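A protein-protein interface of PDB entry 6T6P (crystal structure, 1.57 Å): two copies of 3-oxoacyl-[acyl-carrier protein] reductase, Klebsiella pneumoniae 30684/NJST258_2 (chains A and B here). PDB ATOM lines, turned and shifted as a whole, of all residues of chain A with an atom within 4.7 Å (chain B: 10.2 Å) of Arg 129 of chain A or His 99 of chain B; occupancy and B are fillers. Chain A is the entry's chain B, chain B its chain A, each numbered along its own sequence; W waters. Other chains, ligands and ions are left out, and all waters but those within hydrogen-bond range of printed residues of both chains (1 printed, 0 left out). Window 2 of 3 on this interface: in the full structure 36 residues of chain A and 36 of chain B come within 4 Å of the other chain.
CB of Ala 125 of chain A touches CD2 of Leu 98 of chain B, at 3.7 Å. His 99 of chain B touches Ile 126 of chain A (CB to CG1, 3.8 Å).
Of the 13 printed residues of chain A, 4 touch a printed residue of chain B. Hydrophobic or aromatic side chains of chain A within 4 Å of the printed part of chain B: Ala 125 and Ile 126. Hydrophobic or aromatic side chains of chain B within 4 Å of the printed part of chain A: Leu 98 and His 99.
Water W1 lies within hydrogen-bond range of the side-chain amide oxygen of Gln 122 of chain A (2.7 Å), the backbone carbonyl oxygen of Leu 101 of chain B (2.9 Å) and the backbone NH of Glu 103 of chain B (3.2 Å).
No position is printed for both chains.
Of the printed residues of chain B, Arg 129 of chain A touches His 99. His 99 of chain B touches two residues of chain A. Ala 125 of chain A touches just one residue of chain B: Leu 98 (3.7 Å). Ile 126 of chain A touches one residue of chain B. No residue of chain B comes within 4 Å of Glu 130 of chain A. Of the printed residues of chain A, Leu 98 of chain B touches Gln 122 (2.9 Å) and Ala 125 (3.7 Å). Of the printed residues of chain B, Gln 122 of chain A touches Leu 98 and Leu 101. Of the printed residues of chain A, Leu 101 of chain B touches Gln 122. Ala 96 of chain B touches none of the printed residues of chain A. Gly 132 of chain A touches none of the printed residues of chain B. The nearest printed residue of chain A that does not touch Leu 98 of chain B is Leu 171 of chain A (4.2 Å).
NH1 of Arg 129 of chain A is in salt-bridge range of OE2 of Glu 130 of chain A, at 3.4 Å.
O of Leu 98 of chain B is in hydrogen-bond range of NE2 of Gln 122 of chain A (2.9 Å). A ring nitrogen (NE2) of His 99 of chain B lies close to the guanidinium group of Arg 129 of chain A, 3.4 Å away. The side-chain amide nitrogen of Gln 122 of chain A sits at hydrogen-bond distance from the backbone carbonyl oxygen of Leu 101 of chain B.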
ATOM      1  N   GLN A 122      17.460 -18.783 -11.523  1.00  0.00           N
ATOM      2  CA  GLN A 122      17.196 -17.746 -12.489  1.00  0.00           C
ATOM      3  C   GLN A 122      15.974 -16.908 -12.098  1.00  0.00           C
ATOM      4  O   GLN A 122      16.004 -15.665 -12.164  1.00  0.00           O
ATOM      5  CB  GLN A 122      17.034 -18.319 -13.880  1.00  0.00           C
ATOM      6  CG  GLN A 122      16.657 -17.310 -14.937  1.00  0.00           C
ATOM      7  CD  GLN A 122      16.742 -17.903 -16.321  1.00  0.00           C
ATOM      8  OE1 GLN A 122      15.933 -18.810 -16.684  1.00  0.00           O
ATOM      9  NE2 GLN A 122      17.706 -17.426 -17.112  1.00  0.00           N
ATOM     10  N   ALA A 124      14.763 -16.512  -9.118  1.00  0.00           N
ATOM     11  CA  ALA A 124      15.126 -15.719  -7.938  1.00  0.00           C
ATOM     12  C   ALA A 124      15.974 -14.519  -8.334  1.00  0.00           C
ATOM     13  O   ALA A 124      15.746 -13.398  -7.903  1.00  0.00           O
ATOM     14  CB  ALA A 124      15.834 -16.590  -6.912  1.00  0.00           C
ATOM     15  N   ALA A 125      16.977 -14.751  -9.176  1.00  0.00           N
ATOM     16  CA  ALA A 125      17.888 -13.678  -9.572  1.00  0.00           C
ATOM     17  C   ALA A 125      17.209 -12.544 -10.263  1.00  0.00           C
ATOM     18  O   ALA A 125      17.540 -11.375 -10.012  1.00  0.00           O
ATOM     19  CB  ALA A 125      18.987 -14.249 -10.485  1.00  0.00           C
ATOM     20  N   ILE A 126      16.252 -12.833 -11.161  1.00  0.00           N
ATOM     21  CA  ILE A 126      15.570 -11.786 -11.923  1.00  0.00           C
ATOM     22  C   ILE A 126      14.928 -10.806 -10.903  1.00  0.00           C
ATOM     23  O   ILE A 126      14.932  -9.588 -11.110  1.00  0.00           O
ATOM     24  CB  ILE A 126      14.477 -12.422 -12.809  1.00  0.00           C
ATOM     25  CG1 ILE A 126      15.128 -13.077 -13.987  1.00  0.00           C
ATOM     26  CG2 ILE A 126      13.484 -11.367 -13.317  1.00  0.00           C
ATOM     27  CD1 ILE A 126      14.250 -14.142 -14.719  1.00  0.00           C
ATOM     28  N   ARG A 127      14.308 -11.374  -9.892  1.00  0.00           N
ATOM     29  CA  ARG A 127      13.589 -10.610  -8.877  1.00  0.00           C
ATOM     30  C   ARG A 127      14.526  -9.929  -7.882  1.00  0.00           C
ATOM     31  O   ARG A 127      14.381  -8.713  -7.593  1.00  0.00           O
ATOM     32  CB  ARG A 127      12.644 -11.538  -8.144  1.00  0.00           C
ATOM     33  CG  ARG A 127      11.449 -11.982  -9.021  1.00  0.00           C
ATOM     34  CD  ARG A 127      10.777 -13.176  -8.358  1.00  0.00           C
ATOM     35  NE  ARG A 127       9.506 -13.485  -9.024  1.00  0.00           N
ATOM     36  CZ  ARG A 127       9.392 -14.190 -10.129  1.00  0.00           C
ATOM     37  NH1 ARG A 127      10.448 -14.755 -10.706  1.00  0.00           N
ATOM     38  NH2 ARG A 127       8.164 -14.371 -10.631  1.00  0.00           N
ATOM     39  N   MET A 128      15.444 -10.706  -7.349  1.00  0.00           N
ATOM     40  CA  MET A 128      16.293 -10.212  -6.254  1.00  0.00           C
ATOM     41  C   MET A 128      17.220  -9.108  -6.717  1.00  0.00           C
ATOM     42  O   MET A 128      17.490  -8.147  -5.937  1.00  0.00           O
ATOM     43  CB  MET A 128      17.096 -11.347  -5.625  1.00  0.00           C
ATOM     44  CG  MET A 128      16.250 -12.335  -4.890  1.00  0.00           C
ATOM     45  SD  MET A 128      17.180 -13.777  -4.371  1.00  0.00           S
ATOM     46  CE  MET A 128      15.917 -14.674  -3.454  1.00  0.00           C
ATOM     47  N   ARG A 129      17.711  -9.191  -7.948  1.00  0.00           N
ATOM     48  CA  ARG A 129      18.605  -8.149  -8.405  1.00  0.00           C
ATOM     49  C   ARG A 129      17.901  -6.834  -8.571  1.00  0.00           C
ATOM     50  O   ARG A 129      18.539  -5.807  -8.420  1.00  0.00           O
ATOM     51  CB  ARG A 129      19.361  -8.544  -9.688  1.00  0.00           C
ATOM     52  CG  ARG A 129      18.564  -8.519 -10.914  1.00  0.00           C
ATOM     53  CD  ARG A 129      19.349  -9.318 -11.985  1.00  0.00           C
ATOM     54  NE  ARG A 129      20.576  -8.605 -12.391  1.00  0.00           N
ATOM     55  CZ  ARG A 129      20.584  -7.552 -13.164  1.00  0.00           C
ATOM     56  NH1 ARG A 129      19.446  -7.035 -13.661  1.00  0.00           N
ATOM     57  NH2 ARG A 129      21.759  -7.009 -13.441  1.00  0.00           N
ATOM     58  N   GLU A 130      16.612  -6.850  -8.880  1.00  0.00           N
ATOM     59  CA  GLU A 130      15.823  -5.601  -9.004  1.00  0.00           C
ATOM     60  C   GLU A 130      15.479  -5.023  -7.657  1.00  0.00           C
ATOM     61  O   GLU A 130      15.381  -3.792  -7.511  1.00  0.00           O
ATOM     62  CB  GLU A 130      14.527  -5.881  -9.726  1.00  0.00           C
ATOM     63  CG  GLU A 130      14.744  -6.318 -11.139  1.00  0.00           C
ATOM     64  CD  GLU A 130      15.525  -5.325 -11.953  1.00  0.00           C
ATOM     65  OE1 GLU A 130      15.179  -4.102 -11.881  1.00  0.00           O
ATOM     66  OE2 GLU A 130      16.482  -5.771 -12.666  1.00  0.00           O
ATOM     67  N   ARG A 131      15.267  -5.878  -6.687  1.00  0.00           N
ATOM     68  CA  ARG A 131      14.889  -5.461  -5.355  1.00  0.00           C
ATOM     69  C   ARG A 131      16.070  -5.071  -4.482  1.00  0.00           C
ATOM     70  O   ARG A 131      15.890  -4.405  -3.488  1.00  0.00           O
ATOM     71  CB  ARG A 131      14.052  -6.556  -4.693  1.00  0.00           C
ATOM     72  CG  ARG A 131      12.691  -6.711  -5.404  1.00  0.00           C
ATOM     73  CD  ARG A 131      12.038  -8.072  -5.126  1.00  0.00           C
ATOM     74  NE  ARG A 131      10.828  -8.300  -5.944  1.00  0.00           N
ATOM     75  CZ  ARG A 131      10.177  -9.464  -6.069  1.00  0.00           C
ATOM     76  NH1 ARG A 131      10.553 -10.489  -5.414  1.00  0.00           N
ATOM     77  NH2 ARG A 131       9.080  -9.554  -6.825  1.00  0.00           N
ATOM     78  N   GLY A 132      17.265  -5.510  -4.838  1.00  0.00           N
ATOM     79  CA  GLY A 132      18.466  -5.153  -4.080  1.00  0.00           C
ATOM     80  C   GLY A 132      18.714  -5.925  -2.819  1.00  0.00           C
ATOM     81  O   GLY A 132      19.420  -5.467  -1.928  1.00  0.00           O
ATOM     82  N   LEU A 171      25.765 -11.450  -8.621  1.00  0.00           N
ATOM     83  CA  LEU A 171      24.693 -10.912  -7.811  1.00  0.00           C
ATOM     84  C   LEU A 171      25.115 -10.233  -6.510  1.00  0.00           C
ATOM     85  O   LEU A 171      24.325  -9.492  -5.908  1.00  0.00           O
ATOM     86  CB  LEU A 171      23.681 -11.997  -7.455  1.00  0.00           C
ATOM     87  CG  LEU A 171      22.936 -12.610  -8.651  1.00  0.00           C
ATOM     88  CD1 LEU A 171      22.147 -13.837  -8.172  1.00  0.00           C
ATOM     89  CD2 LEU A 171      22.031 -11.591  -9.314  1.00  0.00           C
ATOM     90  N   LYS A 174      24.499  -6.607  -6.060  1.00  0.00           N
ATOM     91  CA  LYS A 174      23.066  -6.282  -5.952  1.00  0.00           C
ATOM     92  C   LYS A 174      22.489  -6.593  -4.581  1.00  0.00           C
ATOM     93  O   LYS A 174      21.255  -6.598  -4.431  1.00  0.00           O
ATOM     94  CB  LYS A 174      22.281  -7.085  -7.009  1.00  0.00           C
ATOM     95  CG  LYS A 174      22.790  -6.973  -8.415  1.00  0.00           C
ATOM     96  CD  LYS A 174      22.624  -5.594  -8.961  1.00  0.00           C
ATOM     97  CE  LYS A 174      22.991  -5.521 -10.434  1.00  0.00           C
ATOM     98  NZ  LYS A 174      22.676  -4.175 -10.890  1.00  0.00           N
ATOM     99  N   VAL A 176      22.695  -9.580  -2.953  1.00  0.00           N
ATOM    100  CA  VAL A 176      22.264 -10.945  -2.836  1.00  0.00           C
ATOM    101  C   VAL A 176      23.457 -11.829  -2.448  1.00  0.00           C
ATOM    102  O   VAL A 176      24.545 -11.625  -2.978  1.00  0.00           O
ATOM    103  CB  VAL A 176      21.720 -11.398  -4.183  1.00  0.00           C
ATOM    104  CG1 VAL A 176      21.253 -12.851  -4.178  1.00  0.00           C
ATOM    105  CG2 VAL A 176      20.570 -10.471  -4.595  1.00  0.00           C
ATOM    106  N   ASP B  95      27.516 -17.846 -23.695  1.00  0.00           N
ATOM    107  CA  ASP B  95      27.537 -17.096 -22.424  1.00  0.00           C
ATOM    108  C   ASP B  95      26.346 -16.138 -22.330  1.00  0.00           C
ATOM    109  O   ASP B  95      25.854 -15.581 -23.339  1.00  0.00           O
ATOM    110  CB  ASP B  95      28.843 -16.306 -22.305  1.00  0.00           C
ATOM    111  CG  ASP B  95      30.063 -17.161 -22.155  1.00  0.00           C
ATOM    112  OD1 ASP B  95      30.041 -18.385 -22.029  1.00  0.00           O
ATOM    113  OD2 ASP B  95      31.167 -16.584 -22.073  1.00  0.00           O
ATOM    114  N   ALA B  96      25.923 -15.899 -21.095  1.00  0.00           N
ATOM    115  CA  ALA B  96      24.886 -14.967 -20.768  1.00  0.00           C
ATOM    116  C   ALA B  96      24.787 -14.844 -19.249  1.00  0.00           C
ATOM    117  O   ALA B  96      25.069 -15.823 -18.560  1.00  0.00           O
ATOM    118  CB  ALA B  96      23.530 -15.438 -21.266  1.00  0.00           C
ATOM    119  N   MET B  97      24.372 -13.671 -18.810  1.00  0.00           N
ATOM    120  CA  MET B  97      24.116 -13.450 -17.368  1.00  0.00           C
ATOM    121  C   MET B  97      23.003 -14.406 -16.891  1.00  0.00           C
ATOM    122  O   MET B  97      22.126 -14.770 -17.672  1.00  0.00           O
ATOM    123  CB  MET B  97      23.767 -12.032 -17.071  1.00  0.00           C
ATOM    124  CG  MET B  97      24.826 -11.050 -17.484  1.00  0.00           C
ATOM    125  SD  MET B  97      26.382 -11.203 -16.603  1.00  0.00           S
ATOM    126  CE  MET B  97      25.883 -10.431 -15.076  1.00  0.00           C
ATOM    127  N   LEU B  98      23.047 -14.765 -15.596  1.00  0.00           N
ATOM    128  CA  LEU B  98      22.069 -15.733 -15.053  1.00  0.00           C
ATOM    129  C   LEU B  98      20.629 -15.328 -15.313  1.00  0.00           C
ATOM    130  O   LEU B  98      19.826 -16.175 -15.655  1.00  0.00           O
ATOM    131  CB  LEU B  98      22.328 -15.907 -13.546  1.00  0.00           C
ATOM    132  CG  LEU B  98      21.272 -16.652 -12.719  1.00  0.00           C
ATOM    133  CD1 LEU B  98      21.175 -18.062 -13.184  1.00  0.00           C
ATOM    134  CD2 LEU B  98      21.650 -16.623 -11.258  1.00  0.00           C
ATOM    135  N   HIS B  99      20.326 -14.058 -15.203  1.00  0.00           N
ATOM    136  CA  HIS B  99      18.937 -13.550 -15.358  1.00  0.00           C
ATOM    137  C   HIS B  99      18.472 -13.474 -16.823  1.00  0.00           C
ATOM    138  O   HIS B  99      17.303 -13.208 -17.074  1.00  0.00           O
ATOM    139  CB  HIS B  99      18.745 -12.222 -14.640  1.00  0.00           C
ATOM    140  CG  HIS B  99      19.579 -11.095 -15.173  1.00  0.00           C
ATOM    141  ND1 HIS B  99      20.958 -11.054 -15.016  1.00  0.00           N
ATOM    142  CD2 HIS B  99      19.236  -9.985 -15.849  1.00  0.00           C
ATOM    143  CE1 HIS B  99      21.399  -9.935 -15.560  1.00  0.00           C
ATOM    144  NE2 HIS B  99      20.384  -9.278 -16.071  1.00  0.00           N
ATOM    145  N   LYS B 100      19.392 -13.705 -17.761  1.00  0.00           N
ATOM    146  CA  LYS B 100      19.130 -13.585 -19.201  1.00  0.00           C
ATOM    147  C   LYS B 100      19.349 -14.881 -19.989  1.00  0.00           C
ATOM    148  O   LYS B 100      18.917 -14.938 -21.120  1.00  0.00           O
ATOM    149  CB  LYS B 100      20.033 -12.507 -19.817  1.00  0.00           C
ATOM    150  CG  LYS B 100      19.737 -11.120 -19.306  1.00  0.00           C
ATOM    151  CD  LYS B 100      20.704 -10.124 -19.940  1.00  0.00           C
ATOM    152  CE  LYS B 100      20.299  -8.711 -19.726  1.00  0.00           C
ATOM    153  NZ  LYS B 100      21.300  -7.782 -20.389  1.00  0.00           N
ATOM    154  N   LEU B 101      19.918 -15.898 -19.388  1.00  0.00           N
ATOM    155  CA  LEU B 101      20.319 -17.108 -20.116  1.00  0.00           C
ATOM    156  C   LEU B 101      19.070 -17.856 -20.607  1.00  0.00           C
ATOM    157  O   LEU B 101      18.177 -18.194 -19.840  1.00  0.00           O
ATOM    158  CB  LEU B 101      21.146 -18.011 -19.243  1.00  0.00           C
ATOM    159  CG  LEU B 101      21.519 -19.372 -19.828  1.00  0.00           C
ATOM    160  CD1 LEU B 101      22.413 -19.156 -21.038  1.00  0.00           C
ATOM    161  CD2 LEU B 101      22.228 -20.235 -18.799  1.00  0.00           C
ATOM    162  N   THR B 102      18.960 -18.062 -21.929  1.00  0.00           N
ATOM    163  CA  THR B 102      17.813 -18.743 -22.443  1.00  0.00           C
ATOM    164  C   THR B 102      17.911 -20.239 -22.136  1.00  0.00           C
ATOM    165  O   THR B 102      18.978 -20.817 -21.968  1.00  0.00           O
ATOM    166  CB  THR B 102      17.639 -18.574 -23.975  1.00  0.00           C
ATOM    167  OG1 THR B 102      18.719 -19.242 -24.661  1.00  0.00           O
ATOM    168  CG2 THR B 102      17.577 -17.079 -24.345  1.00  0.00           C
ATOM    169  N   GLU B 103      16.744 -20.864 -22.129  1.00  0.00           N
ATOM    170  CA  GLU B 103      16.727 -22.289 -21.931  1.00  0.00           C
ATOM    171  C   GLU B 103      17.511 -23.048 -23.026  1.00  0.00           C
ATOM    172  O   GLU B 103      18.221 -24.033 -22.740  1.00  0.00           O
ATOM    173  CB  GLU B 103      15.260 -22.724 -21.843  1.00  0.00           C
ATOM    174  CG  GLU B 103      15.088 -24.123 -21.345  1.00  0.00           C
ATOM    175  CD  GLU B 103      13.663 -24.536 -21.138  1.00  0.00           C
ATOM    176  OE1 GLU B 103      12.687 -23.730 -21.350  1.00  0.00           O
ATOM    177  OE2 GLU B 103      13.563 -25.762 -20.806  1.00  0.00           O
ATOM    178  N   VAL B 148      31.784 -14.681 -14.247  1.00  0.00           N
ATOM    179  CA  VAL B 148      30.664 -13.843 -14.692  1.00  0.00           C
ATOM    180  C   VAL B 148      30.246 -14.226 -16.119  1.00  0.00           C
ATOM    181  O   VAL B 148      31.110 -14.381 -17.019  1.00  0.00           O
ATOM    182  CB  VAL B 148      31.028 -12.354 -14.616  1.00  0.00           C
ATOM    183  CG1 VAL B 148      29.989 -11.508 -15.288  1.00  0.00           C
ATOM    184  CG2 VAL B 148      31.177 -11.925 -13.169  1.00  0.00           C
ATOM    185  N   GLY B 149      28.938 -14.372 -16.328  1.00  0.00           N
ATOM    186  CA  GLY B 149      28.384 -14.655 -17.655  1.00  0.00           C
ATOM    187  C   GLY B 149      28.409 -16.113 -18.044  1.00  0.00           C
ATOM    188  O   GLY B 149      28.043 -16.449 -19.158  1.00  0.00           O
ATOM    189  N   GLN B 150      28.828 -17.018 -17.135  1.00  0.00           N
ATOM    190  CA  GLN B 150      29.073 -18.405 -17.489  1.00  0.00           C
ATOM    191  C   GLN B 150      28.341 -19.379 -16.570  1.00  0.00           C
ATOM    192  O   GLN B 150      28.860 -20.432 -16.227  1.00  0.00           O
ATOM    193  CB  GLN B 150      30.567 -18.672 -17.518  1.00  0.00           C
ATOM    194  CG  GLN B 150      31.202 -17.898 -18.673  1.00  0.00           C
ATOM    195  CD  GLN B 150      32.621 -18.358 -18.991  1.00  0.00           C
ATOM    196  OE1 GLN B 150      33.349 -18.840 -18.143  1.00  0.00           O
ATOM    197  NE2 GLN B 150      33.010 -18.190 -20.220  1.00  0.00           N
ATOM    198  N   THR B 151      27.086 -19.064 -16.247  1.00  0.00           N
ATOM    199  CA  THR B 151      26.289 -20.046 -15.468  1.00  0.00           C
ATOM    200  C   THR B 151      26.322 -21.444 -16.098  1.00  0.00           C
ATOM    201  O   THR B 151      26.610 -22.449 -15.411  1.00  0.00           O
ATOM    202  CB  THR B 151      24.848 -19.545 -15.313  1.00  0.00           C
ATOM    203  OG1 THR B 151      24.797 -18.404 -14.476  1.00  0.00           O
ATOM    204  CG2 THR B 151      23.949 -20.649 -14.717  1.00  0.00           C
ATOM    205  N   ASN B 152      25.992 -21.521 -17.377  1.00  0.00           N
ATOM    206  CA  ASN B 152      25.966 -22.805 -18.083  1.00  0.00           C
ATOM    207  C   ASN B 152      27.353 -23.421 -18.234  1.00  0.00           C
ATOM    208  O   ASN B 152      27.537 -24.609 -17.990  1.00  0.00           O
ATOM    209  CB  ASN B 152      25.215 -22.713 -19.446  1.00  0.00           C
ATOM    210  CG  ASN B 152      25.687 -21.589 -20.374  1.00  0.00           C
ATOM    211  OD1 ASN B 152      26.598 -20.832 -20.057  1.00  0.00           O
ATOM    212  ND2 ASN B 152      25.085 -21.527 -21.556  1.00  0.00           N
HETATM  213  O   HOH W   1      15.926 -19.850 -19.181  1.00  0.00           O
